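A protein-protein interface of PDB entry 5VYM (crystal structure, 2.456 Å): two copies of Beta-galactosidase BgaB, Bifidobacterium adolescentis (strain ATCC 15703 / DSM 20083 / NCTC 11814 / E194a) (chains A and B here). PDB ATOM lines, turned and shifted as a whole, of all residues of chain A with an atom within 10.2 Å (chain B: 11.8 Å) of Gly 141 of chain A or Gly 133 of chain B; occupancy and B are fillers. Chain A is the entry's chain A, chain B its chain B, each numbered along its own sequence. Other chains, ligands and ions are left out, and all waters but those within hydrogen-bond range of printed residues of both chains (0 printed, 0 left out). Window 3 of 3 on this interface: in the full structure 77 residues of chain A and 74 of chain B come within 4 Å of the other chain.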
ATOM      1  N   PRO A 140       5.317 -24.029  18.438  1.00  0.00           N
ATOM      2  CA  PRO A 140       6.271 -22.935  18.303  1.00  0.00           C
ATOM      3  C   PRO A 140       7.700 -23.455  18.145  1.00  0.00           C
ATOM      4  O   PRO A 140       8.656 -22.676  18.111  1.00  0.00           O
ATOM      5  CB  PRO A 140       6.175 -22.006  19.498  1.00  0.00           C
ATOM      6  N   GLY A 141       7.840 -24.774  18.046  1.00  0.00           N
ATOM      7  CA  GLY A 141       9.144 -25.382  17.872  1.00  0.00           C
ATOM      8  C   GLY A 141       9.753 -25.895  19.162  1.00  0.00           C
ATOM      9  O   GLY A 141       9.522 -27.045  19.550  1.00  0.00           O
ATOM     10  N   GLU A 142      10.541 -25.055  19.830  1.00  0.00           N
ATOM     11  CA  GLU A 142      11.176 -25.407  21.094  1.00  0.00           C
ATOM     12  C   GLU A 142      11.020 -24.248  22.064  1.00  0.00           C
ATOM     13  O   GLU A 142      11.265 -23.095  21.700  1.00  0.00           O
ATOM     14  CB  GLU A 142      12.657 -25.747  20.899  1.00  0.00           C
ATOM     15  CG  GLU A 142      13.420 -25.969  22.193  1.00  0.00           C
ATOM     16  CD  GLU A 142      14.816 -26.510  21.960  1.00  0.00           C
ATOM     17  OE1 GLU A 142      15.018 -27.225  20.955  1.00  0.00           O
ATOM     18  OE2 GLU A 142      15.712 -26.219  22.779  1.00  0.00           O
ATOM     19  N   ILE A 143      10.618 -24.557  23.296  1.00  0.00           N
ATOM     20  CA  ILE A 143      10.316 -23.553  24.308  1.00  0.00           C
ATOM     21  C   ILE A 143      11.269 -23.726  25.483  1.00  0.00           C
ATOM     22  O   ILE A 143      11.695 -24.839  25.805  1.00  0.00           O
ATOM     23  CB  ILE A 143       8.845 -23.650  24.772  1.00  0.00           C
ATOM     24  CG1 ILE A 143       7.909 -23.598  23.568  1.00  0.00           C
ATOM     25  CG2 ILE A 143       8.496 -22.530  25.735  1.00  0.00           C
ATOM     26  CD1 ILE A 143       8.076 -22.359  22.720  1.00  0.00           C
ATOM     27  N   ARG A 144      11.606 -22.609  26.118  1.00  0.00           N
ATOM     28  CA  ARG A 144      12.438 -22.589  27.310  1.00  0.00           C
ATOM     29  C   ARG A 144      11.564 -22.395  28.545  1.00  0.00           C
ATOM     30  O   ARG A 144      10.484 -21.800  28.477  1.00  0.00           O
ATOM     31  CB  ARG A 144      13.489 -21.479  27.214  1.00  0.00           C
ATOM     32  CG  ARG A 144      14.618 -21.570  28.229  1.00  0.00           C
ATOM     33  CD  ARG A 144      15.882 -20.885  27.721  1.00  0.00           C
ATOM     34  NE  ARG A 144      16.519 -21.634  26.639  1.00  0.00           N
ATOM     35  CZ  ARG A 144      16.404 -21.337  25.348  1.00  0.00           C
ATOM     36  NH1 ARG A 144      15.678 -20.296  24.964  1.00  0.00           N
ATOM     37  NH2 ARG A 144      17.021 -22.080  24.438  1.00  0.00           N
ATOM     38  N   THR A 158      14.823 -26.625  28.454  1.00  0.00           N
ATOM     39  CA  THR A 158      14.032 -26.511  27.239  1.00  0.00           C
ATOM     40  C   THR A 158      13.132 -27.728  27.087  1.00  0.00           C
ATOM     41  O   THR A 158      13.367 -28.782  27.684  1.00  0.00           O
ATOM     42  CB  THR A 158      14.919 -26.368  25.994  1.00  0.00           C
ATOM     43  OG1 THR A 158      15.851 -27.455  25.944  1.00  0.00           O
ATOM     44  CG2 THR A 158      15.678 -25.050  26.027  1.00  0.00           C
ATOM     45  N   THR A 159      12.092 -27.566  26.274  1.00  0.00           N
ATOM     46  CA  THR A 159      11.174 -28.648  25.952  1.00  0.00           C
ATOM     47  C   THR A 159      10.787 -28.549  24.485  1.00  0.00           C
ATOM     48  O   THR A 159      10.763 -27.461  23.903  1.00  0.00           O
ATOM     49  CB  THR A 159       9.913 -28.619  26.828  1.00  0.00           C
ATOM     50  OG1 THR A 159       9.060 -29.718  26.480  1.00  0.00           O
ATOM     51  CG2 THR A 159       9.155 -27.313  26.635  1.00  0.00           C
ATOM     52  N   ARG A 160      10.495 -29.702  23.890  1.00  0.00           N
ATOM     53  CA  ARG A 160      10.090 -29.778  22.495  1.00  0.00           C
ATOM     54  C   ARG A 160       8.713 -30.400  22.323  1.00  0.00           C
ATOM     55  O   ARG A 160       8.237 -30.520  21.189  1.00  0.00           O
ATOM     56  CB  ARG A 160      11.134 -30.563  21.689  1.00  0.00           C
ATOM     57  CG  ARG A 160      12.555 -30.061  21.916  1.00  0.00           C
ATOM     58  CD  ARG A 160      13.599 -30.963  21.282  1.00  0.00           C
ATOM     59  NE  ARG A 160      13.647 -30.822  19.829  1.00  0.00           N
ATOM     60  CZ  ARG A 160      14.588 -31.359  19.060  1.00  0.00           C
ATOM     61  NH1 ARG A 160      15.564 -32.071  19.606  1.00  0.00           N
ATOM     62  NH2 ARG A 160      14.556 -31.181  17.747  1.00  0.00           N
ATOM     63  N   LEU A 161       8.065 -30.799  23.416  1.00  0.00           N
ATOM     64  CA  LEU A 161       6.694 -31.295  23.388  1.00  0.00           C
ATOM     65  C   LEU A 161       6.053 -30.931  24.717  1.00  0.00           C
ATOM     66  O   LEU A 161       6.475 -31.431  25.763  1.00  0.00           O
ATOM     67  CB  LEU A 161       6.651 -32.807  23.156  1.00  0.00           C
ATOM     68  CG  LEU A 161       5.260 -33.425  22.993  1.00  0.00           C
ATOM     69  CD1 LEU A 161       4.575 -32.882  21.747  1.00  0.00           C
ATOM     70  CD2 LEU A 161       5.336 -34.944  22.953  1.00  0.00           C
ATOM     71  N   TRP A 162       5.050 -30.056  24.678  1.00  0.00           N
ATOM     72  CA  TRP A 162       4.442 -29.523  25.887  1.00  0.00           C
ATOM     73  C   TRP A 162       2.932 -29.453  25.718  1.00  0.00           C
ATOM     74  O   TRP A 162       2.423 -29.295  24.606  1.00  0.00           O
ATOM     75  CB  TRP A 162       4.982 -28.126  26.220  1.00  0.00           C
ATOM     76  CG  TRP A 162       4.661 -27.104  25.166  1.00  0.00           C
ATOM     77  CD1 TRP A 162       3.601 -26.243  25.152  1.00  0.00           C
ATOM     78  CD2 TRP A 162       5.402 -26.845  23.967  1.00  0.00           C
ATOM     79  NE1 TRP A 162       3.638 -25.463  24.021  1.00  0.00           N
ATOM     80  CE2 TRP A 162       4.734 -25.813  23.276  1.00  0.00           C
ATOM     81  CE3 TRP A 162       6.566 -27.385  23.411  1.00  0.00           C
ATOM     82  CZ2 TRP A 162       5.192 -25.311  22.060  1.00  0.00           C
ATOM     83  CZ3 TRP A 162       7.018 -26.884  22.202  1.00  0.00           C
ATOM     84  CH2 TRP A 162       6.332 -25.859  21.539  1.00  0.00           C
ATOM     85  N   GLN A 163       2.223 -29.569  26.838  1.00  0.00           N
ATOM     86  CA  GLN A 163       0.787 -29.336  26.857  1.00  0.00           C
ATOM     87  C   GLN A 163       0.523 -27.837  26.868  1.00  0.00           C
ATOM     88  O   GLN A 163       1.091 -27.104  27.683  1.00  0.00           O
ATOM     89  CB  GLN A 163       0.151 -30.003  28.077  1.00  0.00           C
ATOM     90  CG  GLN A 163      -1.298 -29.610  28.324  1.00  0.00           C
ATOM     91  CD  GLN A 163      -2.260 -30.208  27.317  1.00  0.00           C
ATOM     92  OE1 GLN A 163      -1.897 -31.089  26.538  1.00  0.00           O
ATOM     93  NE2 GLN A 163      -3.499 -29.731  27.331  1.00  0.00           N
ATOM     94  N   ASN A 164      -0.338 -27.382  25.959  1.00  0.00           N
ATOM     95  CA  ASN A 164      -0.562 -25.954  25.772  1.00  0.00           C
ATOM     96  C   ASN A 164      -1.727 -25.413  26.590  1.00  0.00           C
ATOM     97  O   ASN A 164      -1.683 -24.254  27.020  1.00  0.00           O
ATOM     98  CB  ASN A 164      -0.802 -25.653  24.289  1.00  0.00           C
ATOM     99  CG  ASN A 164      -1.007 -24.176  24.020  1.00  0.00           C
ATOM    100  OD1 ASN A 164      -0.046 -23.419  23.888  1.00  0.00           O
ATOM    101  ND2 ASN A 164      -2.266 -23.759  23.936  1.00  0.00           N
ATOM    102  N   TYR A 179       6.612 -21.339  31.118  1.00  0.00           N
ATOM    103  CA  TYR A 179       7.263 -21.157  29.828  1.00  0.00           C
ATOM    104  C   TYR A 179       7.522 -19.675  29.598  1.00  0.00           C
ATOM    105  O   TYR A 179       6.625 -18.845  29.778  1.00  0.00           O
ATOM    106  CB  TYR A 179       6.400 -21.724  28.702  1.00  0.00           C
ATOM    107  CG  TYR A 179       5.954 -23.153  28.916  1.00  0.00           C
ATOM    108  CD1 TYR A 179       6.861 -24.203  28.846  1.00  0.00           C
ATOM    109  CD2 TYR A 179       4.622 -23.453  29.175  1.00  0.00           C
ATOM    110  CE1 TYR A 179       6.456 -25.510  29.038  1.00  0.00           C
ATOM    111  CE2 TYR A 179       4.208 -24.756  29.367  1.00  0.00           C
ATOM    112  CZ  TYR A 179       5.129 -25.780  29.298  1.00  0.00           C
ATOM    113  OH  TYR A 179       4.718 -27.079  29.490  1.00  0.00           O
ATOM    114  N   GLU A 182      11.268 -15.524  23.991  1.00  0.00           N
ATOM    115  CA  GLU A 182      10.701 -15.044  22.735  1.00  0.00           C
ATOM    116  C   GLU A 182       9.953 -16.156  22.009  1.00  0.00           C
ATOM    117  O   GLU A 182       8.903 -15.912  21.402  1.00  0.00           O
ATOM    118  CB  GLU A 182      11.802 -14.467  21.846  1.00  0.00           C
ATOM    119  N   GLU A 183      10.478 -17.382  22.059  1.00  0.00           N
ATOM    120  CA  GLU A 183       9.794 -18.504  21.426  1.00  0.00           C
ATOM    121  C   GLU A 183       8.495 -18.842  22.145  1.00  0.00           C
ATOM    122  O   GLU A 183       7.530 -19.280  21.506  1.00  0.00           O
ATOM    123  CB  GLU A 183      10.710 -19.729  21.383  1.00  0.00           C
ATOM    124  CG  GLU A 183      12.003 -19.532  20.602  1.00  0.00           C
ATOM    125  CD  GLU A 183      13.075 -18.816  21.403  1.00  0.00           C
ATOM    126  OE1 GLU A 183      12.863 -18.585  22.613  1.00  0.00           O
ATOM    127  OE2 GLU A 183      14.130 -18.483  20.822  1.00  0.00           O
ATOM    128  N   ALA A 184       8.450 -18.648  23.465  1.00  0.00           N
ATOM    129  CA  ALA A 184       7.223 -18.912  24.209  1.00  0.00           C
ATOM    130  C   ALA A 184       6.160 -17.858  23.929  1.00  0.00           C
ATOM    131  O   ALA A 184       4.963 -18.170  23.934  1.00  0.00           O
ATOM    132  CB  ALA A 184       7.519 -18.982  25.706  1.00  0.00           C
ATOM    133  N   ASP A 185       6.573 -16.612  23.684  1.00  0.00           N
ATOM    134  CA  ASP A 185       5.609 -15.554  23.403  1.00  0.00           C
ATOM    135  C   ASP A 185       5.027 -15.676  22.000  1.00  0.00           C
ATOM    136  O   ASP A 185       3.912 -15.203  21.752  1.00  0.00           O
ATOM    137  CB  ASP A 185       6.265 -14.185  23.589  1.00  0.00           C
ATOM    138  N   GLU A 186       5.759 -16.305  21.075  1.00  0.00           N
ATOM    139  CA  GLU A 186       5.264 -16.446  19.709  1.00  0.00           C
ATOM    140  C   GLU A 186       4.032 -17.339  19.645  1.00  0.00           C
ATOM    141  O   GLU A 186       3.200 -17.179  18.744  1.00  0.00           O
ATOM    142  CB  GLU A 186       6.368 -16.996  18.804  1.00  0.00           C
ATOM    143  N   TRP A 187       3.896 -18.276  20.582  1.00  0.00           N
ATOM    144  CA  TRP A 187       2.734 -19.149  20.657  1.00  0.00           C
ATOM    145  C   TRP A 187       1.743 -18.703  21.724  1.00  0.00           C
ATOM    146  O   TRP A 187       0.855 -19.478  22.098  1.00  0.00           O
ATOM    147  CB  TRP A 187       3.172 -20.592  20.912  1.00  0.00           C
ATOM    148  N   LEU A 189       2.214 -18.363  24.832  1.00  0.00           N
ATOM    149  CA  LEU A 189       2.391 -19.235  25.987  1.00  0.00           C
ATOM    150  C   LEU A 189       3.338 -18.630  27.018  1.00  0.00           C
ATOM    151  O   LEU A 189       3.859 -19.350  27.876  1.00  0.00           O
ATOM    152  CB  LEU A 189       2.895 -20.611  25.547  1.00  0.00           C
ATOM    153  N   GLY A 209       3.957 -30.527  32.875  1.00  0.00           N
ATOM    154  CA  GLY A 209       3.245 -30.238  31.648  1.00  0.00           C
ATOM    155  C   GLY A 209       4.008 -30.390  30.352  1.00  0.00           C
ATOM    156  O   GLY A 209       3.433 -30.150  29.285  1.00  0.00           O
ATOM    157  N   CYS A 210       5.278 -30.787  30.395  1.00  0.00           N
ATOM    158  CA  CYS A 210       6.087 -30.880  29.187  1.00  0.00           C
ATOM    159  C   CYS A 210       7.042 -32.061  29.287  1.00  0.00           C
ATOM    160  O   CYS A 210       7.280 -32.609  30.367  1.00  0.00           O
ATOM    161  CB  CYS A 210       6.879 -29.589  28.941  1.00  0.00           C
ATOM    162  SG  CYS A 210       7.937 -29.091  30.320  1.00  0.00           S
ATOM    163  N   ASP A 211       7.590 -32.443  28.135  1.00  0.00           N
ATOM    164  CA  ASP A 211       8.613 -33.475  28.077  1.00  0.00           C
ATOM    165  C   ASP A 211       9.980 -32.875  28.370  1.00  0.00           C
ATOM    166  O   ASP A 211      10.305 -31.776  27.911  1.00  0.00           O
ATOM    167  CB  ASP A 211       8.626 -34.149  26.705  1.00  0.00           C
ATOM    168  CG  ASP A 211       9.751 -35.158  26.561  1.00  0.00           C
ATOM    169  OD1 ASP A 211       9.582 -36.312  27.009  1.00  0.00           O
ATOM    170  OD2 ASP A 211      10.812 -34.796  26.008  1.00  0.00           O
ATOM    171  N   PRO B  25      -1.159 -38.579  18.980  1.00  0.00           N
ATOM    172  CA  PRO B  25      -0.806 -37.346  18.253  1.00  0.00           C
ATOM    173  C   PRO B  25       0.690 -37.124  18.069  1.00  0.00           C
ATOM    174  O   PRO B  25       1.066 -36.189  17.350  1.00  0.00           O
ATOM    175  CB  PRO B  25      -1.422 -36.239  19.121  1.00  0.00           C
ATOM    176  CG  PRO B  25      -2.534 -36.907  19.846  1.00  0.00           C
ATOM    177  CD  PRO B  25      -2.058 -38.305  20.116  1.00  0.00           C
ATOM    178  N   SER B  26       1.550 -37.933  18.684  1.00  0.00           N
ATOM    179  CA  SER B  26       2.987 -37.751  18.532  1.00  0.00           C
ATOM    180  C   SER B  26       3.695 -39.064  18.829  1.00  0.00           C
ATOM    181  O   SER B  26       3.356 -39.752  19.795  1.00  0.00           O
ATOM    182  CB  SER B  26       3.512 -36.646  19.457  1.00  0.00           C
ATOM    183  OG  SER B  26       4.928 -36.577  19.417  1.00  0.00           O
ATOM    184  N   MET B  27       4.679 -39.403  17.992  1.00  0.00           N
ATOM    185  CA  MET B  27       5.471 -40.603  18.223  1.00  0.00           C
ATOM    186  C   MET B  27       6.403 -40.454  19.418  1.00  0.00           C
ATOM    187  O   MET B  27       6.931 -41.460  19.904  1.00  0.00           O
ATOM    188  CB  MET B  27       6.280 -40.952  16.973  1.00  0.00           C
ATOM    189  CG  MET B  27       5.445 -41.190  15.722  1.00  0.00           C
ATOM    190  SD  MET B  27       4.328 -42.601  15.845  1.00  0.00           S
ATOM    191  CE  MET B  27       2.768 -41.788  16.191  1.00  0.00           C
ATOM    192  N   LYS B  28       6.621 -39.226  19.896  1.00  0.00           N
ATOM    193  CA  LYS B  28       7.433 -39.019  21.088  1.00  0.00           C
ATOM    194  C   LYS B  28       6.756 -39.560  22.341  1.00  0.00           C
ATOM    195  O   LYS B  28       7.441 -39.836  23.332  1.00  0.00           O
ATOM    196  CB  LYS B  28       7.746 -37.529  21.247  1.00  0.00           C
ATOM    197  CG  LYS B  28       8.766 -37.198  22.331  1.00  0.00           C
ATOM    198  CD  LYS B  28      10.095 -37.889  22.078  1.00  0.00           C
ATOM    199  CE  LYS B  28      11.171 -37.377  23.027  1.00  0.00           C
ATOM    200  NZ  LYS B  28      10.810 -37.583  24.459  1.00  0.00           N
ATOM    201  N   LEU B  29       5.434 -39.720  22.319  1.00  0.00           N
ATOM    202  CA  LEU B  29       4.714 -40.322  23.436  1.00  0.00           C
ATOM    203  C   LEU B  29       5.108 -41.788  23.553  1.00  0.00           C
ATOM    204  O   LEU B  29       4.707 -42.616  22.728  1.00  0.00           O
ATOM    205  CB  LEU B  29       3.210 -40.171  23.235  1.00  0.00           C
ATOM    206  CG  LEU B  29       2.671 -38.742  23.271  1.00  0.00           C
ATOM    207  CD1 LEU B  29       1.192 -38.712  22.912  1.00  0.00           C
ATOM    208  CD2 LEU B  29       2.910 -38.120  24.639  1.00  0.00           C
ATOM    209  N   TYR B  94       2.246 -35.045  31.754  1.00  0.00           N
ATOM    210  CA  TYR B  94       1.285 -34.340  30.911  1.00  0.00           C
ATOM    211  C   TYR B  94       0.427 -35.298  30.092  1.00  0.00           C
ATOM    212  O   TYR B  94      -0.714 -34.966  29.750  1.00  0.00           O
ATOM    213  CB  TYR B  94       2.013 -33.358  29.991  1.00  0.00           C
ATOM    214  CG  TYR B  94       2.971 -34.005  29.014  1.00  0.00           C
ATOM    215  CD1 TYR B  94       4.266 -34.333  29.393  1.00  0.00           C
ATOM    216  CD2 TYR B  94       2.583 -34.278  27.707  1.00  0.00           C
ATOM    217  CE1 TYR B  94       5.145 -34.923  28.502  1.00  0.00           C
ATOM    218  CE2 TYR B  94       3.455 -34.866  26.809  1.00  0.00           C
ATOM    219  CZ  TYR B  94       4.734 -35.186  27.212  1.00  0.00           C
ATOM    220  OH  TYR B  94       5.606 -35.771  26.321  1.00  0.00           O
ATOM    221  N   PHE B 129      -6.713 -32.424  25.650  1.00  0.00           N
ATOM    222  CA  PHE B 129      -5.316 -32.724  25.372  1.00  0.00           C
ATOM    223  C   PHE B 129      -4.872 -31.977  24.119  1.00  0.00           C
ATOM    224  O   PHE B 129      -5.489 -32.100  23.057  1.00  0.00           O
ATOM    225  CB  PHE B 129      -5.141 -34.234  25.201  1.00  0.00           C
ATOM    226  CG  PHE B 129      -3.710 -34.686  25.131  1.00  0.00           C
ATOM    227  CD1 PHE B 129      -2.823 -34.392  26.153  1.00  0.00           C
ATOM    228  CD2 PHE B 129      -3.263 -35.440  24.058  1.00  0.00           C
ATOM    229  CE1 PHE B 129      -1.508 -34.822  26.093  1.00  0.00           C
ATOM    230  CE2 PHE B 129      -1.952 -35.873  23.993  1.00  0.00           C
ATOM    231  CZ  PHE B 129      -1.074 -35.565  25.012  1.00  0.00           C
ATOM    232  N   ASN B 130      -3.805 -31.187  24.250  1.00  0.00           N
ATOM    233  CA  ASN B 130      -3.379 -30.293  23.170  1.00  0.00           C
ATOM    234  C   ASN B 130      -1.876 -30.052  23.327  1.00  0.00           C
ATOM    235  O   ASN B 130      -1.454 -29.173  24.080  1.00  0.00           O
ATOM    236  CB  ASN B 130      -4.165 -28.991  23.202  1.00  0.00           C
ATOM    237  CG  ASN B 130      -3.667 -27.986  22.186  1.00  0.00           C
ATOM    238  OD1 ASN B 130      -3.186 -28.354  21.115  1.00  0.00           O
ATOM    239  ND2 ASN B 130      -3.776 -26.705  22.522  1.00  0.00           N
ATOM    240  N   ILE B 131      -1.084 -30.835  22.600  1.00  0.00           N
ATOM    241  CA  ILE B 131       0.369 -30.746  22.660  1.00  0.00           C
ATOM    242  C   ILE B 131       0.885 -30.039  21.416  1.00  0.00           C
ATOM    243  O   ILE B 131       0.306 -30.141  20.327  1.00  0.00           O
ATOM    244  CB  ILE B 131       1.020 -32.136  22.817  1.00  0.00           C
ATOM    245  CG1 ILE B 131       0.510 -33.094  21.738  1.00  0.00           C
ATOM    246  CG2 ILE B 131       0.761 -32.692  24.208  1.00  0.00           C
ATOM    247  CD1 ILE B 131       1.112 -34.480  21.824  1.00  0.00           C
ATOM    248  N   LEU B 132       1.988 -29.314  21.580  1.00  0.00           N
ATOM    249  CA  LEU B 132       2.624 -28.589  20.493  1.00  0.00           C
ATOM    250  C   LEU B 132       4.110 -28.918  20.465  1.00  0.00           C
ATOM    251  O   LEU B 132       4.682 -29.384  21.453  1.00  0.00           O
ATOM    252  CB  LEU B 132       2.428 -27.073  20.632  1.00  0.00           C
ATOM    253  CG  LEU B 132       0.989 -26.561  20.556  1.00  0.00           C
ATOM    254  CD1 LEU B 132       0.941 -25.061  20.796  1.00  0.00           C
ATOM    255  CD2 LEU B 132       0.362 -26.915  19.214  1.00  0.00           C
ATOM    256  N   GLY B 133       4.728 -28.666  19.315  1.00  0.00           N
ATOM    257  CA  GLY B 133       6.146 -28.922  19.138  1.00  0.00           C
ATOM    258  C   GLY B 133       6.441 -30.026  18.141  1.00  0.00           C
ATOM    259  O   GLY B 133       7.551 -30.127  17.619  1.00  0.00           O
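The backbone NH of Asn 130 of chain B sits at hydrogen-bond distance from the side-chain amide oxygen of Gln 163 of chain A (3.0 Å).
The side-chain amino group of Lys 28 of chain B is in salt-bridge range of the side-chain carboxylate of Asp 211 of chain A.
The backbone NH (N) of Asn 164 of chain A is in hydrogen-bond range of the backbone carbonyl oxygen (O) of Asn 130 of chain B (2.8 Å).
The backbone carbonyl oxygen of Trp 162 of chain A lies within hydrogen-bond range of the backbone NH of Leu 132 of chain B (3.1 Å).
OG of Ser 26 of chain B sits close to N of Lys 28 of chain B (3.2 Å).
OH of Tyr 179 of chain A lies within hydrogen-bond range of O of Gly 209 of chain A (3.3 Å).
The backbone NH of Asp 211 of chain A is in hydrogen-bond range of the backbone carbonyl oxygen of Leu 161 of chain A, at 2.8 Å.
OG1 of Thr 159 of chain A sits at hydrogen-bond distance from O of Asp 211 of chain A (2.8 Å).
O of Gly 209 of chain A sits at hydrogen-bond distance from N of Gln 163 of chain A, 2.8 Å away.
The side-chain hydroxyl (OG1) of Thr 159 of chain A lies within hydrogen-bond range of the backbone carbonyl oxygen (O) of Leu 161 of chain A.
CA of Gly 133 of chain B touches O of Gly 141 of chain A (3.9 Å).
O of Arg 160 of chain A touches O of Leu 132 of chain B, 3.7 Å away.
Leu 161 of chain A touches Ser 26 of chain B.
Leu 161 of chain A touches Lys 28 of chain B.
CA of Leu 161 of chain A touches O of Leu 132 of chain B, 3.4 Å away.
Trp 162 of chain A touches Asn 130 of chain B.
Trp 162 of chain A touches Gly 133 of chain B.
O of Gly 209 of chain A touches CB of Tyr 94 of chain B, at 3.6 Å.
Tyr 94 of chain B touches Cys 210 of chain A.
CB of Asp 211 of chain A touches OH of Tyr 94 of chain B (3.4 Å).
Of chain B, only Gly 133 comes within 4 Å of Gly 141 of chain A.
Gly 133 of chain B touches three residues of chain A.
No residue of chain B comes within 4 Å of Glu 142 of chain A.
Ile 143 of chain A touches none of the printed residues of chain B.
Of chain B, only Ser 26 (3.9 Å), Lys 28 (3.9 Å), Tyr 94 (3.5 Å), Ile 131 (3.8 Å) and Leu 132 (3.4 Å) come within 4 Å of Leu 161 of chain A.
Trp 162 of chain A touches just these residues of chain B: Asn 130 (3.9 Å), Ile 131 (3.2 Å), Leu 132 (3.1 Å) and Gly 133 (3.8 Å).
Leu 132 of chain B touches four residues of chain A.
Of the printed residues of chain B, Arg 160 of chain A touches Leu 132 and Gly 133.
Of the printed residues of chain B, Gly 209 of chain A touches Tyr 94.
The nearest residue of chain B that does not touch Gly 141 of chain A is Leu 132 of chain B (5.7 Å).
The nearest residue of chain A that does not touch Gly 133 of chain B is Pro 140 of chain A (4.8 Å).
The nearest printed residue of chain A that does not touch Lys 28 of chain B is Arg 160 of chain A (6.8 Å).
Hydrophobic or aromatic side chains of chain B that line the printed part of chain A: Tyr 94, Phe 129, Ile 131 and Leu 132.
Of the 23 printed residues of chain A, 9 touch a printed residue of chain B.
Hydrophobic or aromatic side chains of chain A within 4 Å of the printed part of chain B: Leu 161 and Trp 162.
Among the printed residues, 21 pairs touch across the chains.
Among the printed residues, Asp or Glu carboxylates within 4 Å of a Lys or Arg side-chain nitrogen of the other chain: Asp 211 of chain A with Lys 28 of chain B (3.1 Å).
No position is printed for both chains.
Of the 21 pairs that touch across the chains among the printed residues, none has its exchanged pair printed and touching as well.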
